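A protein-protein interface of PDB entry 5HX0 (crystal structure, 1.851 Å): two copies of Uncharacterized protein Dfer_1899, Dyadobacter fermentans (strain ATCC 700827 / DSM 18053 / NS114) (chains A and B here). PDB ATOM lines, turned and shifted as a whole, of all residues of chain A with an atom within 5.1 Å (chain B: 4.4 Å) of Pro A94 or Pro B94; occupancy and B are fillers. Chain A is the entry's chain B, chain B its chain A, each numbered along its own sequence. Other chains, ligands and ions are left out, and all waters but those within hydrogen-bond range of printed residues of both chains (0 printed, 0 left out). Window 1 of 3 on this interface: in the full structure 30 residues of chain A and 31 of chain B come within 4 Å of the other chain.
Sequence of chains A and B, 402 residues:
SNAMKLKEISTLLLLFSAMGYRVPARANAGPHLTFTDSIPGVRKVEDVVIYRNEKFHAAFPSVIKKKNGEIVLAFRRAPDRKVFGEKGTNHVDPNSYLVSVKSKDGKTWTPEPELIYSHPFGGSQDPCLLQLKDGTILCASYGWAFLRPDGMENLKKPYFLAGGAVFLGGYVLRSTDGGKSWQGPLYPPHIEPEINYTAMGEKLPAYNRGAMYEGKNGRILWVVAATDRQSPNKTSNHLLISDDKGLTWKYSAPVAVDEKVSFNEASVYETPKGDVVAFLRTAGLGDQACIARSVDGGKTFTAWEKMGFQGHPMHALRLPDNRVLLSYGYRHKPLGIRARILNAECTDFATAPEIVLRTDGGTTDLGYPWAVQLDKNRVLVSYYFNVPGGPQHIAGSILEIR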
ATOM      1  N   VAL A  92     -29.079   4.900   6.591  1.00  0.00           N
ATOM      2  CA  VAL A  92     -29.354   3.597   5.978  1.00  0.00           C
ATOM      3  C   VAL A  92     -28.075   2.771   5.966  1.00  0.00           C
ATOM      4  O   VAL A  92     -26.982   3.296   5.710  1.00  0.00           O
ATOM      5  CB  VAL A  92     -29.943   3.725   4.553  1.00  0.00           C
ATOM      6  CG1 VAL A  92     -31.220   4.557   4.573  1.00  0.00           C
ATOM      7  CG2 VAL A  92     -28.945   4.323   3.624  1.00  0.00           C
ATOM      8  N   ASP A  93     -28.218   1.485   6.244  1.00  0.00           N
ATOM      9  CA  ASP A  93     -27.119   0.527   6.316  1.00  0.00           C
ATOM     10  C   ASP A  93     -27.741  -0.864   6.338  1.00  0.00           C
ATOM     11  O   ASP A  93     -28.616  -1.128   7.174  1.00  0.00           O
ATOM     12  CB  ASP A  93     -26.264   0.784   7.567  1.00  0.00           C
ATOM     13  CG  ASP A  93     -24.909   0.079   7.524  1.00  0.00           C
ATOM     14  OD1 ASP A  93     -24.878  -1.156   7.306  1.00  0.00           O
ATOM     15  OD2 ASP A  93     -23.865   0.766   7.718  1.00  0.00           O
ATOM     16  N   PRO A  94     -27.338  -1.776   5.447  1.00  0.00           N
ATOM     17  CA  PRO A  94     -27.915  -3.135   5.492  1.00  0.00           C
ATOM     18  C   PRO A  94     -27.708  -3.836   6.820  1.00  0.00           C
ATOM     19  O   PRO A  94     -28.522  -4.693   7.188  1.00  0.00           O
ATOM     20  CB  PRO A  94     -27.183  -3.874   4.361  1.00  0.00           C
ATOM     21  CG  PRO A  94     -25.840  -3.090   4.229  1.00  0.00           C
ATOM     22  CD  PRO A  94     -26.255  -1.660   4.454  1.00  0.00           C
ATOM     23  N   ASN A  95     -26.652  -3.493   7.568  1.00  0.00           N
ATOM     24  CA  ASN A  95     -26.384  -4.153   8.835  1.00  0.00           C
ATOM     25  C   ASN A  95     -26.857  -3.354  10.049  1.00  0.00           C
ATOM     26  O   ASN A  95     -26.354  -3.558  11.156  1.00  0.00           O
ATOM     27  CB  ASN A  95     -24.890  -4.491   8.927  1.00  0.00           C
ATOM     28  CG  ASN A  95     -24.463  -5.440   7.817  1.00  0.00           C
ATOM     29  OD1 ASN A  95     -23.874  -5.024   6.814  1.00  0.00           O
ATOM     30  ND2 ASN A  95     -24.822  -6.715   7.961  1.00  0.00           N
ATOM     31  N   SER A  96     -27.861  -2.496   9.897  1.00  0.00           N
ATOM     32  CA  SER A  96     -28.456  -1.864  11.076  1.00  0.00           C
ATOM     33  C   SER A  96     -29.423  -2.856  11.696  1.00  0.00           C
ATOM     34  O   SER A  96     -30.305  -3.393  11.002  1.00  0.00           O
ATOM     35  CB  SER A  96     -29.151  -0.540  10.734  1.00  0.00           C
ATOM     36  OG  SER A  96     -30.260  -0.702   9.851  1.00  0.00           O
ATOM     37  N   TYR A  97     -29.222  -3.139  12.983  1.00  0.00           N
ATOM     38  CA  TYR A  97     -29.971  -4.148  13.711  1.00  0.00           C
ATOM     39  C   TYR A  97     -30.715  -3.487  14.871  1.00  0.00           C
ATOM     40  O   TYR A  97     -30.343  -2.420  15.342  1.00  0.00           O
ATOM     41  CB  TYR A  97     -29.054  -5.251  14.268  1.00  0.00           C
ATOM     42  CG  TYR A  97     -28.184  -5.967  13.243  1.00  0.00           C
ATOM     43  CD1 TYR A  97     -28.606  -6.145  11.929  1.00  0.00           C
ATOM     44  CD2 TYR A  97     -26.932  -6.469  13.607  1.00  0.00           C
ATOM     45  CE1 TYR A  97     -27.801  -6.810  10.994  1.00  0.00           C
ATOM     46  CE2 TYR A  97     -26.132  -7.136  12.690  1.00  0.00           C
ATOM     47  CZ  TYR A  97     -26.566  -7.303  11.385  1.00  0.00           C
ATOM     48  OH  TYR A  97     -25.748  -7.961  10.473  1.00  0.00           O
ATOM     49  N   GLY A 122     -32.532  -6.825   4.885  1.00  0.00           N
ATOM     50  CA  GLY A 122     -31.954  -5.487   4.842  1.00  0.00           C
ATOM     51  C   GLY A 122     -31.794  -4.914   6.238  1.00  0.00           C
ATOM     52  O   GLY A 122     -31.813  -5.646   7.232  1.00  0.00           O
ATOM     53  N   GLY A 123     -31.627  -3.591   6.288  1.00  0.00           N
ATOM     54  CA  GLY A 123     -31.370  -2.911   7.550  1.00  0.00           C
ATOM     55  C   GLY A 123     -32.657  -2.467   8.219  1.00  0.00           C
ATOM     56  O   GLY A 123     -33.626  -2.143   7.550  1.00  0.00           O
ATOM     57  N   PHE A 146     -31.002  -3.172  -0.111  1.00  0.00           N
ATOM     58  CA  PHE A 146     -29.887  -2.674  -0.898  1.00  0.00           C
ATOM     59  C   PHE A 146     -29.779  -3.533  -2.148  1.00  0.00           C
ATOM     60  O   PHE A 146     -29.405  -4.708  -2.067  1.00  0.00           O
ATOM     61  CB  PHE A 146     -28.616  -2.681  -0.035  1.00  0.00           C
ATOM     62  CG  PHE A 146     -28.715  -1.710   1.117  1.00  0.00           C
ATOM     63  CD1 PHE A 146     -29.468  -2.030   2.249  1.00  0.00           C
ATOM     64  CD2 PHE A 146     -28.161  -0.454   1.023  1.00  0.00           C
ATOM     65  CE1 PHE A 146     -29.623  -1.129   3.275  1.00  0.00           C
ATOM     66  CE2 PHE A 146     -28.291   0.456   2.064  1.00  0.00           C
ATOM     67  CZ  PHE A 146     -29.026   0.116   3.186  1.00  0.00           C
ATOM     68  N   ASP B  93     -23.349 -11.262   0.439  1.00  0.00           N
ATOM     69  CA  ASP B  93     -24.560 -10.495   0.710  1.00  0.00           C
ATOM     70  C   ASP B  93     -24.406  -9.881   2.095  1.00  0.00           C
ATOM     71  O   ASP B  93     -24.099 -10.619   3.035  1.00  0.00           O
ATOM     72  CB  ASP B  93     -25.804 -11.402   0.645  1.00  0.00           C
ATOM     73  CG  ASP B  93     -27.119 -10.605   0.627  1.00  0.00           C
ATOM     74  OD1 ASP B  93     -27.350  -9.785   1.546  1.00  0.00           O
ATOM     75  OD2 ASP B  93     -27.921 -10.793  -0.324  1.00  0.00           O
ATOM     76  N   PRO B  94     -24.592  -8.560   2.281  1.00  0.00           N
ATOM     77  CA  PRO B  94     -24.420  -7.996   3.638  1.00  0.00           C
ATOM     78  C   PRO B  94     -25.334  -8.636   4.666  1.00  0.00           C
ATOM     79  O   PRO B  94     -24.988  -8.688   5.853  1.00  0.00           O
ATOM     80  CB  PRO B  94     -24.746  -6.502   3.452  1.00  0.00           C
ATOM     81  CG  PRO B  94     -25.661  -6.464   2.206  1.00  0.00           C
ATOM     82  CD  PRO B  94     -25.080  -7.550   1.317  1.00  0.00           C
ATOM     83  N   ASN B  95     -26.481  -9.170   4.239  1.00  0.00           N
ATOM     84  CA  ASN B  95     -27.436  -9.734   5.188  1.00  0.00           C
ATOM     85  C   ASN B  95     -27.381 -11.260   5.272  1.00  0.00           C
ATOM     86  O   ASN B  95     -28.373 -11.875   5.664  1.00  0.00           O
ATOM     87  CB  ASN B  95     -28.845  -9.265   4.844  1.00  0.00           C
ATOM     88  CG  ASN B  95     -28.995  -7.768   5.026  1.00  0.00           C
ATOM     89  OD1 ASN B  95     -29.006  -7.005   4.055  1.00  0.00           O
ATOM     90  ND2 ASN B  95     -29.039  -7.334   6.284  1.00  0.00           N
ATOM     91  N   SER B  96     -26.245 -11.882   4.943  1.00  0.00           N
ATOM     92  CA  SER B  96     -26.100 -13.314   5.178  1.00  0.00           C
ATOM     93  C   SER B  96     -25.781 -13.535   6.655  1.00  0.00           C
ATOM     94  O   SER B  96     -24.830 -12.945   7.200  1.00  0.00           O
ATOM     95  CB  SER B  96     -25.025 -13.932   4.273  1.00  0.00           C
ATOM     96  OG  SER B  96     -23.709 -13.449   4.573  1.00  0.00           O
ATOM     97  N   GLY B 122     -21.055  -6.750   8.488  1.00  0.00           N
ATOM     98  CA  GLY B 122     -21.327  -7.265   7.154  1.00  0.00           C
ATOM     99  C   GLY B 122     -21.907  -8.673   7.187  1.00  0.00           C
ATOM    100  O   GLY B 122     -22.472  -9.106   8.195  1.00  0.00           O
ATOM    101  N   GLY B 123     -21.745  -9.371   6.044  1.00  0.00           N
ATOM    102  CA  GLY B 123     -22.304 -10.707   5.865  1.00  0.00           C
ATOM    103  C   GLY B 123     -21.355 -11.795   6.343  1.00  0.00           C
ATOM    104  O   GLY B 123     -20.128 -11.653   6.276  1.00  0.00           O
ATOM    105  N   PHE B 146     -19.255  -4.304   2.926  1.00  0.00           N
ATOM    106  CA  PHE B 146     -19.756  -3.657   1.717  1.00  0.00           C
ATOM    107  C   PHE B 146     -19.520  -2.164   1.862  1.00  0.00           C
ATOM    108  O   PHE B 146     -20.196  -1.499   2.644  1.00  0.00           O
ATOM    109  CB  PHE B 146     -21.229  -4.010   1.484  1.00  0.00           C
ATOM    110  CG  PHE B 146     -21.423  -5.483   1.195  1.00  0.00           C
ATOM    111  CD1 PHE B 146     -21.386  -6.413   2.224  1.00  0.00           C
ATOM    112  CD2 PHE B 146     -21.549  -5.935  -0.107  1.00  0.00           C
ATOM    113  CE1 PHE B 146     -21.503  -7.797   1.955  1.00  0.00           C
ATOM    114  CE2 PHE B 146     -21.684  -7.299  -0.383  1.00  0.00           C
ATOM    115  CZ  PHE B 146     -21.662  -8.231   0.661  1.00  0.00           C
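ND2 of Asn A95 sits at hydrogen-bond distance from O of Pro B94 (2.9 Å). The side-chain amide nitrogen (ND2) of Asn B95 lies within hydrogen-bond range of the backbone carbonyl oxygen (O) of Pro A94 (2.8 Å). The backbone carbonyl oxygen (O) of Gly A122 lies within hydrogen-bond range of the side-chain amide nitrogen (ND2) of Asn B95. O of Gly B122 sits at hydrogen-bond distance from ND2 of Asn A95, at 3.4 Å.
N of Asn B95 is in hydrogen-bond range of OD1 of Asp B93. The backbone carbonyl oxygen of Pro B94 lies within hydrogen-bond range of the backbone NH of Gly B123. The side-chain carboxylate (OD1) of Asp A93 lies within hydrogen-bond range of the backbone NH (N) of Asn A95 (2.9 Å). O of Pro A94 lies close to N of Gly A123 (3.4 Å). ND2 of Asn A95 is in hydrogen-bond range of OH of Tyr A97.
Of the 9 printed residues of chain A, 3 touch a printed residue of chain B. Hydrophobic or aromatic side chains of chain B within 4 Å of the printed part of chain A: Pro B94. Among the printed residues, 5 pairs touch across the chains.
Pro A94 touches just these residues of chain B: Pro B94 and Asn B95. Pro B94 touches just these residues of chain A: Pro A94 and Asn A95. Of the printed residues of chain B, Gly A122 touches Asn B95. Of the printed residues of chain B, Asn A95 touches Pro B94 and Gly B122. Of the printed residues of chain A, Gly B122 touches Asn A95. Printed residues of chain A within 4 Å of Asn B95: Pro A94 and Gly A122. The nearest printed residue of chain B that does not touch Pro A94 is Phe B146 (5.4 Å).
Pro A94 touches its own counterpart, Pro B94. Pro A94 touches Asn B95, and with the chains exchanged Asn A95 touches Pro B94. Asn A95 touches Gly B122, and with the chains exchanged Gly A122 touches Asn B95. Of the 5 pairs that touch across the chains among the printed residues, 5 have their exchanged pair printed and touching as well.
Pro B94 touches Pro A94.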
